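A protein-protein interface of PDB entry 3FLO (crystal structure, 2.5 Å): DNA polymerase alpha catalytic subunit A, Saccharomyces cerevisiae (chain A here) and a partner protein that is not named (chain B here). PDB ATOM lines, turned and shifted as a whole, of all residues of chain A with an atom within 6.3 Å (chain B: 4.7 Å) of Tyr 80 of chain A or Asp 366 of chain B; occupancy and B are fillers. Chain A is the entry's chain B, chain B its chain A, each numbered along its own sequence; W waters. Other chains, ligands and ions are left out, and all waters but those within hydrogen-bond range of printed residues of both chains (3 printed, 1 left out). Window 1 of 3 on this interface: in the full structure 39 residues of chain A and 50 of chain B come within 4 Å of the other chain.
OH of Tyr 79 of chain A sits at hydrogen-bond distance from O of Met 5 of chain B, 3.4 Å away.
The side-chain carboxylate of Asp 366 of chain B is in hydrogen-bond range of the side-chain hydroxyl of Ser 77 of chain A.
The backbone NH (N) of Gln 7 of chain B sits at hydrogen-bond distance from the side-chain hydroxyl (OH) of Tyr 79 of chain A (3.0 Å).
The side-chain hydroxyl (OG1) of Thr 243 of chain B sits at hydrogen-bond distance from the side-chain carboxylate (OD2) of Asp 366 of chain B (2.9 Å).
The backbone NH (N) of Tyr 253 of chain B lies within hydrogen-bond range of the backbone carbonyl oxygen (O) of Asp 366 of chain B, at 2.8 Å.
Among the printed residues, pairs that only touch across the chains: Ile 76 of chain A with Met 5 of chain B, Ser 77 of chain A with Ser 363 of chain B, Ser 77 of chain A with Gly 364 of chain B, Tyr 80 of chain A with Met 5 of chain B, Tyr 80 of chain A with Ala 252 of chain B, Tyr 80 of chain A with Asp 366 of chain B and Tyr 80 of chain A with Leu 367 of chain B.
Of chain B, only Met 5 (3.4 Å), Ala 252 (3.5 Å), Asp 366 (3.8 Å) and Leu 367 (3.8 Å) come within 4 Å of Tyr 80 of chain A.
Printed residues of chain A within 4 Å of Gln 7 of chain B: Tyr 79.
Of the printed residues of chain A, Ser 363 of chain B touches Ser 77.
Of the printed residues of chain A, Gly 364 of chain B touches Ser 77.
Printed residues of chain A within 4 Å of Leu 367 of chain B: Tyr 80.
Asp 368 of chain B touches none of the printed residues of chain A.
The nearest residue of chain B that does not touch Tyr 80 of chain A is Asp 368 of chain B (4.03 Å).
The nearest printed residue of chain A that does not touch Leu 367 of chain B is Ala 81 of chain A (6.0 Å).
Of the 13 printed residues of chain B, 7 touch a printed residue of chain A.
Printed residues of chain B that touch a printed residue of chain A: Met 5, Gln 7, Ala 252, Ser 363, Gly 364, Asp 366 and Leu 367.
Of the 12 printed residues of chain A, 4 touch a printed residue of chain B.
Printed residues of chain A that touch a printed residue of chain B: Ile 76, Ser 77, Tyr 79 and Tyr 80.
Hydrophobic or aromatic side chains of chain A within 4 Å of the printed part of chain B: Ile 76, Tyr 79 and Tyr 80.
Among the printed residues, 10 pairs touch across the chains.
Water W3 lies within hydrogen-bond range of the side-chain amide nitrogen (NE2) of Gln 7 of chain B (2.6 Å), the backbone carbonyl oxygen (O) of Leu 367 of chain B (3.1 Å) and the backbone carbonyl oxygen (O) of Tyr 80 of chain A (3.5 Å).
Water W1 lies within hydrogen-bond range of OH of Tyr 80 of chain A and O of Thr 4 of chain B.
Water W2 bridges the backbone NH (N) of Leu 367 of chain B (2.7 Å) and the backbone carbonyl oxygen (O) of Tyr 80 of chain A (3.0 Å).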
ATOM      1  N   HIS A  75      -0.551  14.923 -27.764  1.00  0.00           N
ATOM      2  CA  HIS A  75      -1.849  14.310 -27.998  1.00  0.00           C
ATOM      3  C   HIS A  75      -2.585  14.068 -26.668  1.00  0.00           C
ATOM      4  O   HIS A  75      -3.768  14.266 -26.607  1.00  0.00           O
ATOM      5  CB  HIS A  75      -1.750  12.996 -28.770  1.00  0.00           C
ATOM      6  CG  HIS A  75      -1.612  13.177 -30.237  1.00  0.00           C
ATOM      7  ND1 HIS A  75      -2.704  13.253 -31.081  1.00  0.00           N
ATOM      8  CD2 HIS A  75      -0.510  13.245 -31.036  1.00  0.00           C
ATOM      9  CE1 HIS A  75      -2.285  13.406 -32.327  1.00  0.00           C
ATOM     10  NE2 HIS A  75      -0.960  13.406 -32.330  1.00  0.00           N
ATOM     11  N   ILE A  76      -1.892  13.569 -25.661  1.00  0.00           N
ATOM     12  CA  ILE A  76      -2.532  13.201 -24.433  1.00  0.00           C
ATOM     13  C   ILE A  76      -3.064  14.455 -23.745  1.00  0.00           C
ATOM     14  O   ILE A  76      -4.170  14.443 -23.189  1.00  0.00           O
ATOM     15  CB  ILE A  76      -1.602  12.392 -23.478  1.00  0.00           C
ATOM     16  CG1 ILE A  76      -1.338  10.975 -24.044  1.00  0.00           C
ATOM     17  CG2 ILE A  76      -2.187  12.256 -22.063  1.00  0.00           C
ATOM     18  CD1 ILE A  76      -0.230  10.229 -23.263  1.00  0.00           C
ATOM     19  N   SER A  77      -2.325  15.556 -23.889  1.00  0.00           N
ATOM     20  CA  SER A  77      -2.709  16.855 -23.312  1.00  0.00           C
ATOM     21  C   SER A  77      -3.937  17.417 -24.055  1.00  0.00           C
ATOM     22  O   SER A  77      -4.903  17.858 -23.424  1.00  0.00           O
ATOM     23  CB  SER A  77      -1.532  17.814 -23.339  1.00  0.00           C
ATOM     24  OG  SER A  77      -1.805  19.050 -22.718  1.00  0.00           O
ATOM     25  N   LEU A  78      -3.959  17.334 -25.371  1.00  0.00           N
ATOM     26  CA  LEU A  78      -5.112  17.798 -26.107  1.00  0.00           C
ATOM     27  C   LEU A  78      -6.328  17.021 -25.610  1.00  0.00           C
ATOM     28  O   LEU A  78      -7.380  17.600 -25.325  1.00  0.00           O
ATOM     29  CB  LEU A  78      -4.893  17.574 -27.592  1.00  0.00           C
ATOM     30  CG  LEU A  78      -6.072  17.958 -28.484  1.00  0.00           C
ATOM     31  CD1 LEU A  78      -6.452  19.426 -28.201  1.00  0.00           C
ATOM     32  CD2 LEU A  78      -5.744  17.721 -29.965  1.00  0.00           C
ATOM     33  N   TYR A  79      -6.162  15.706 -25.493  1.00  0.00           N
ATOM     34  CA  TYR A  79      -7.209  14.804 -25.037  1.00  0.00           C
ATOM     35  C   TYR A  79      -7.768  15.206 -23.663  1.00  0.00           C
ATOM     36  O   TYR A  79      -8.973  15.184 -23.461  1.00  0.00           O
ATOM     37  CB  TYR A  79      -6.657  13.382 -24.947  1.00  0.00           C
ATOM     38  CG  TYR A  79      -7.503  12.309 -24.234  1.00  0.00           C
ATOM     39  CD1 TYR A  79      -8.499  11.610 -24.905  1.00  0.00           C
ATOM     40  CD2 TYR A  79      -7.276  11.982 -22.911  1.00  0.00           C
ATOM     41  CE1 TYR A  79      -9.235  10.605 -24.286  1.00  0.00           C
ATOM     42  CE2 TYR A  79      -8.011  10.979 -22.269  1.00  0.00           C
ATOM     43  CZ  TYR A  79      -8.983  10.292 -22.962  1.00  0.00           C
ATOM     44  OH  TYR A  79      -9.712   9.310 -22.325  1.00  0.00           O
ATOM     45  N   TYR A  80      -6.879  15.551 -22.732  1.00  0.00           N
ATOM     46  CA  TYR A  80      -7.296  16.035 -21.432  1.00  0.00           C
ATOM     47  C   TYR A  80      -7.802  17.503 -21.412  1.00  0.00           C
ATOM     48  O   TYR A  80      -8.266  17.960 -20.382  1.00  0.00           O
ATOM     49  CB  TYR A  80      -6.189  15.804 -20.376  1.00  0.00           C
ATOM     50  CG  TYR A  80      -6.152  14.374 -19.900  1.00  0.00           C
ATOM     51  CD1 TYR A  80      -7.164  13.861 -19.111  1.00  0.00           C
ATOM     52  CD2 TYR A  80      -5.125  13.538 -20.250  1.00  0.00           C
ATOM     53  CE1 TYR A  80      -7.139  12.539 -18.686  1.00  0.00           C
ATOM     54  CE2 TYR A  80      -5.078  12.232 -19.837  1.00  0.00           C
ATOM     55  CZ  TYR A  80      -6.080  11.730 -19.066  1.00  0.00           C
ATOM     56  OH  TYR A  80      -6.049  10.407 -18.708  1.00  0.00           O
ATOM     57  N   ALA A  81      -7.737  18.228 -22.522  1.00  0.00           N
ATOM     58  CA  ALA A  81      -8.354  19.541 -22.587  1.00  0.00           C
ATOM     59  C   ALA A  81      -9.879  19.400 -22.506  1.00  0.00           C
ATOM     60  O   ALA A  81     -10.572  20.332 -22.092  1.00  0.00           O
ATOM     61  CB  ALA A  81      -7.959  20.279 -23.847  1.00  0.00           C
ATOM     62  N   GLY A  82     -10.380  18.259 -22.942  1.00  0.00           N
ATOM     63  CA  GLY A  82     -11.752  17.883 -22.749  1.00  0.00           C
ATOM     64  C   GLY A  82     -12.758  18.625 -23.572  1.00  0.00           C
ATOM     65  O   GLY A  82     -13.837  18.929 -23.099  1.00  0.00           O
ATOM     66  N   TRP A  83     -12.402  18.958 -24.791  1.00  0.00           N
ATOM     67  CA  TRP A  83     -13.350  19.575 -25.701  1.00  0.00           C
ATOM     68  C   TRP A  83     -14.505  18.607 -25.976  1.00  0.00           C
ATOM     69  O   TRP A  83     -14.328  17.394 -25.987  1.00  0.00           O
ATOM     70  CB  TRP A  83     -12.688  19.928 -27.025  1.00  0.00           C
ATOM     71  CG  TRP A  83     -11.722  20.986 -26.953  1.00  0.00           C
ATOM     72  CD1 TRP A  83     -10.371  20.856 -26.875  1.00  0.00           C
ATOM     73  CD2 TRP A  83     -12.003  22.379 -26.984  1.00  0.00           C
ATOM     74  NE1 TRP A  83      -9.785  22.103 -26.851  1.00  0.00           N
ATOM     75  CE2 TRP A  83     -10.773  23.054 -26.925  1.00  0.00           C
ATOM     76  CE3 TRP A  83     -13.181  23.119 -27.076  1.00  0.00           C
ATOM     77  CZ2 TRP A  83     -10.676  24.444 -26.946  1.00  0.00           C
ATOM     78  CZ3 TRP A  83     -13.098  24.501 -27.087  1.00  0.00           C
ATOM     79  CH2 TRP A  83     -11.838  25.154 -27.028  1.00  0.00           C
ATOM     80  N   ARG A  96     -15.821  23.427 -23.864  1.00  0.00           N
ATOM     81  CA  ARG A  96     -15.269  22.636 -22.801  1.00  0.00           C
ATOM     82  C   ARG A  96     -16.207  22.615 -21.595  1.00  0.00           C
ATOM     83  O   ARG A  96     -15.939  21.910 -20.619  1.00  0.00           O
ATOM     84  CB  ARG A  96     -13.868  23.149 -22.460  1.00  0.00           C
ATOM     85  CG  ARG A  96     -12.929  22.987 -23.630  1.00  0.00           C
ATOM     86  CD  ARG A  96     -11.635  23.705 -23.431  1.00  0.00           C
ATOM     87  NE  ARG A  96     -10.934  23.188 -22.279  1.00  0.00           N
ATOM     88  CZ  ARG A  96     -10.322  23.951 -21.383  1.00  0.00           C
ATOM     89  NH1 ARG A  96     -10.321  25.276 -21.474  1.00  0.00           N
ATOM     90  NH2 ARG A  96      -9.747  23.380 -20.358  1.00  0.00           N
ATOM     91  N   TYR A 118     -12.115  14.526 -28.758  1.00  0.00           N
ATOM     92  CA  TYR A 118     -11.029  13.565 -28.848  1.00  0.00           C
ATOM     93  C   TYR A 118     -11.424  12.373 -28.037  1.00  0.00           C
ATOM     94  O   TYR A 118     -11.108  12.291 -26.849  1.00  0.00           O
ATOM     95  CB  TYR A 118      -9.707  14.110 -28.247  1.00  0.00           C
ATOM     96  CG  TYR A 118      -8.419  13.489 -28.843  1.00  0.00           C
ATOM     97  CD1 TYR A 118      -8.434  12.276 -29.531  1.00  0.00           C
ATOM     98  CD2 TYR A 118      -7.207  14.127 -28.739  1.00  0.00           C
ATOM     99  CE1 TYR A 118      -7.277  11.736 -30.100  1.00  0.00           C
ATOM    100  CE2 TYR A 118      -6.049  13.581 -29.270  1.00  0.00           C
ATOM    101  CZ  TYR A 118      -6.093  12.389 -29.964  1.00  0.00           C
ATOM    102  OH  TYR A 118      -4.943  11.847 -30.505  1.00  0.00           O
ATOM    103  N   LEU A 123      -7.726   8.404 -29.407  1.00  0.00           N
ATOM    104  CA  LEU A 123      -6.422   8.489 -28.762  1.00  0.00           C
ATOM    105  C   LEU A 123      -5.686   7.165 -28.819  1.00  0.00           C
ATOM    106  O   LEU A 123      -4.492   7.126 -29.106  1.00  0.00           O
ATOM    107  CB  LEU A 123      -6.549   8.921 -27.281  1.00  0.00           C
ATOM    108  CG  LEU A 123      -5.222   9.082 -26.520  1.00  0.00           C
ATOM    109  CD1 LEU A 123      -4.302  10.110 -27.218  1.00  0.00           C
ATOM    110  CD2 LEU A 123      -5.423   9.460 -25.088  1.00  0.00           C
ATOM    111  N   THR B   4      -6.731   3.898 -15.810  1.00  0.00           N
ATOM    112  CA  THR B   4      -6.290   4.034 -17.206  1.00  0.00           C
ATOM    113  C   THR B   4      -6.605   5.446 -17.763  1.00  0.00           C
ATOM    114  O   THR B   4      -7.141   6.301 -17.040  1.00  0.00           O
ATOM    115  CB  THR B   4      -6.965   2.927 -18.088  1.00  0.00           C
ATOM    116  OG1 THR B   4      -6.176   2.677 -19.266  1.00  0.00           O
ATOM    117  CG2 THR B   4      -8.425   3.303 -18.455  1.00  0.00           C
ATOM    118  N   MET B   5      -6.278   5.679 -19.037  1.00  0.00           N
ATOM    119  CA  MET B   5      -6.775   6.861 -19.764  1.00  0.00           C
ATOM    120  C   MET B   5      -8.170   6.608 -20.336  1.00  0.00           C
ATOM    121  O   MET B   5      -8.346   6.274 -21.501  1.00  0.00           O
ATOM    122  CB  MET B   5      -5.813   7.297 -20.854  1.00  0.00           C
ATOM    123  CG  MET B   5      -4.508   7.810 -20.271  1.00  0.00           C
ATOM    124  SD  MET B   5      -3.393   8.535 -21.477  1.00  0.00           S
ATOM    125  CE  MET B   5      -2.766   7.078 -22.367  1.00  0.00           C
ATOM    126  N   GLN B   7     -11.922   8.662 -20.419  1.00  0.00           N
ATOM    127  CA  GLN B   7     -12.718   9.803 -20.041  1.00  0.00           C
ATOM    128  C   GLN B   7     -14.113   9.358 -20.391  1.00  0.00           C
ATOM    129  O   GLN B   7     -14.335   8.843 -21.500  1.00  0.00           O
ATOM    130  CB  GLN B   7     -12.246  11.136 -20.676  1.00  0.00           C
ATOM    131  CG  GLN B   7     -11.159  11.866 -19.767  1.00  0.00           C
ATOM    132  CD  GLN B   7     -11.294  13.400 -19.694  1.00  0.00           C
ATOM    133  OE1 GLN B   7     -11.216  14.084 -20.733  1.00  0.00           O
ATOM    134  NE2 GLN B   7     -11.466  13.954 -18.453  1.00  0.00           N
ATOM    135  N   THR B 243       2.514  17.276 -14.342  1.00  0.00           N
ATOM    136  CA  THR B 243       1.990  16.590 -15.504  1.00  0.00           C
ATOM    137  C   THR B 243       2.876  16.879 -16.734  1.00  0.00           C
ATOM    138  O   THR B 243       2.662  16.315 -17.774  1.00  0.00           O
ATOM    139  CB  THR B 243       0.514  16.966 -15.808  1.00  0.00           C
ATOM    140  OG1 THR B 243       0.442  18.326 -16.260  1.00  0.00           O
ATOM    141  CG2 THR B 243      -0.397  16.747 -14.612  1.00  0.00           C
ATOM    142  N   ALA B 251      -0.094  11.629 -17.241  1.00  0.00           N
ATOM    143  CA  ALA B 251      -0.008  13.046 -17.552  1.00  0.00           C
ATOM    144  C   ALA B 251      -1.356  13.743 -17.393  1.00  0.00           C
ATOM    145  O   ALA B 251      -1.729  14.554 -18.219  1.00  0.00           O
ATOM    146  CB  ALA B 251       0.532  13.205 -18.983  1.00  0.00           C
ATOM    147  N   ALA B 252      -2.089  13.410 -16.347  1.00  0.00           N
ATOM    148  CA  ALA B 252      -3.318  14.133 -15.951  1.00  0.00           C
ATOM    149  C   ALA B 252      -3.269  14.458 -14.452  1.00  0.00           C
ATOM    150  O   ALA B 252      -2.697  13.715 -13.681  1.00  0.00           O
ATOM    151  CB  ALA B 252      -4.552  13.254 -16.264  1.00  0.00           C
ATOM    152  N   TYR B 253      -3.829  15.599 -14.065  1.00  0.00           N
ATOM    153  CA  TYR B 253      -4.084  15.934 -12.635  1.00  0.00           C
ATOM    154  C   TYR B 253      -5.484  15.450 -12.232  1.00  0.00           C
ATOM    155  O   TYR B 253      -6.447  15.722 -12.932  1.00  0.00           O
ATOM    156  CB  TYR B 253      -4.008  17.418 -12.467  1.00  0.00           C
ATOM    157  CG  TYR B 253      -4.175  17.935 -11.044  1.00  0.00           C
ATOM    158  CD1 TYR B 253      -5.393  18.452 -10.619  1.00  0.00           C
ATOM    159  CD2 TYR B 253      -3.095  17.966 -10.147  1.00  0.00           C
ATOM    160  CE1 TYR B 253      -5.538  18.949  -9.348  1.00  0.00           C
ATOM    161  CE2 TYR B 253      -3.238  18.452  -8.867  1.00  0.00           C
ATOM    162  CZ  TYR B 253      -4.465  18.967  -8.472  1.00  0.00           C
ATOM    163  OH  TYR B 253      -4.668  19.471  -7.212  1.00  0.00           O
ATOM    164  N   SER B 363       0.354  22.242 -23.757  1.00  0.00           N
ATOM    165  CA  SER B 363       0.206  21.744 -22.414  1.00  0.00           C
ATOM    166  C   SER B 363      -1.053  22.333 -21.701  1.00  0.00           C
ATOM    167  O   SER B 363      -1.840  23.049 -22.299  1.00  0.00           O
ATOM    168  CB  SER B 363       1.478  22.091 -21.660  1.00  0.00           C
ATOM    169  OG  SER B 363       1.742  23.472 -21.872  1.00  0.00           O
ATOM    170  N   GLY B 364      -1.241  22.004 -20.428  1.00  0.00           N
ATOM    171  CA  GLY B 364      -2.398  22.536 -19.663  1.00  0.00           C
ATOM    172  C   GLY B 364      -2.542  21.949 -18.272  1.00  0.00           C
ATOM    173  O   GLY B 364      -1.759  21.112 -17.865  1.00  0.00           O
ATOM    174  N   ALA B 365      -3.547  22.396 -17.536  1.00  0.00           N
ATOM    175  CA  ALA B 365      -3.906  21.743 -16.274  1.00  0.00           C
ATOM    176  C   ALA B 365      -4.136  20.218 -16.452  1.00  0.00           C
ATOM    177  O   ALA B 365      -3.837  19.433 -15.581  1.00  0.00           O
ATOM    178  CB  ALA B 365      -5.117  22.418 -15.698  1.00  0.00           C
ATOM    179  N   ASP B 366      -4.665  19.818 -17.592  1.00  0.00           N
ATOM    180  CA  ASP B 366      -4.902  18.422 -17.892  1.00  0.00           C
ATOM    181  C   ASP B 366      -5.722  17.783 -16.787  1.00  0.00           C
ATOM    182  O   ASP B 366      -5.302  16.772 -16.203  1.00  0.00           O
ATOM    183  CB  ASP B 366      -3.572  17.606 -18.023  1.00  0.00           C
ATOM    184  CG  ASP B 366      -2.544  18.239 -18.964  1.00  0.00           C
ATOM    185  OD1 ASP B 366      -2.946  18.708 -20.071  1.00  0.00           O
ATOM    186  OD2 ASP B 366      -1.338  18.248 -18.560  1.00  0.00           O
ATOM    187  N   LEU B 367      -6.896  18.337 -16.498  1.00  0.00           N
ATOM    188  CA  LEU B 367      -7.674  17.808 -15.391  1.00  0.00           C
ATOM    189  C   LEU B 367      -8.303  16.510 -15.821  1.00  0.00           C
ATOM    190  O   LEU B 367      -8.844  16.405 -16.902  1.00  0.00           O
ATOM    191  CB  LEU B 367      -8.761  18.768 -14.932  1.00  0.00           C
ATOM    192  CG  LEU B 367      -8.319  20.149 -14.569  1.00  0.00           C
ATOM    193  CD1 LEU B 367      -9.535  20.936 -14.030  1.00  0.00           C
ATOM    194  CD2 LEU B 367      -7.114  20.090 -13.596  1.00  0.00           C
ATOM    195  N   ASP B 368      -8.231  15.517 -14.955  1.00  0.00           N
ATOM    196  CA  ASP B 368      -8.931  14.299 -15.192  1.00  0.00           C
ATOM    197  C   ASP B 368     -10.197  14.376 -14.342  1.00  0.00           C
ATOM    198  O   ASP B 368     -10.186  14.053 -13.160  1.00  0.00           O
ATOM    199  CB  ASP B 368      -8.083  13.123 -14.816  1.00  0.00           C
ATOM    200  CG  ASP B 368      -8.785  11.825 -15.083  1.00  0.00           C
ATOM    201  OD1 ASP B 368      -9.926  11.855 -15.591  1.00  0.00           O
ATOM    202  OD2 ASP B 368      -8.235  10.769 -14.777  1.00  0.00           O
HETATM  203  O   HOH W   1      -8.351   9.390 -18.011  1.00  0.00           O
HETATM  204  O   HOH W   2      -8.182  20.009 -18.200  1.00  0.00           O
HETATM  205  O   HOH W   3     -11.086  16.456 -18.997  1.00  0.00           O
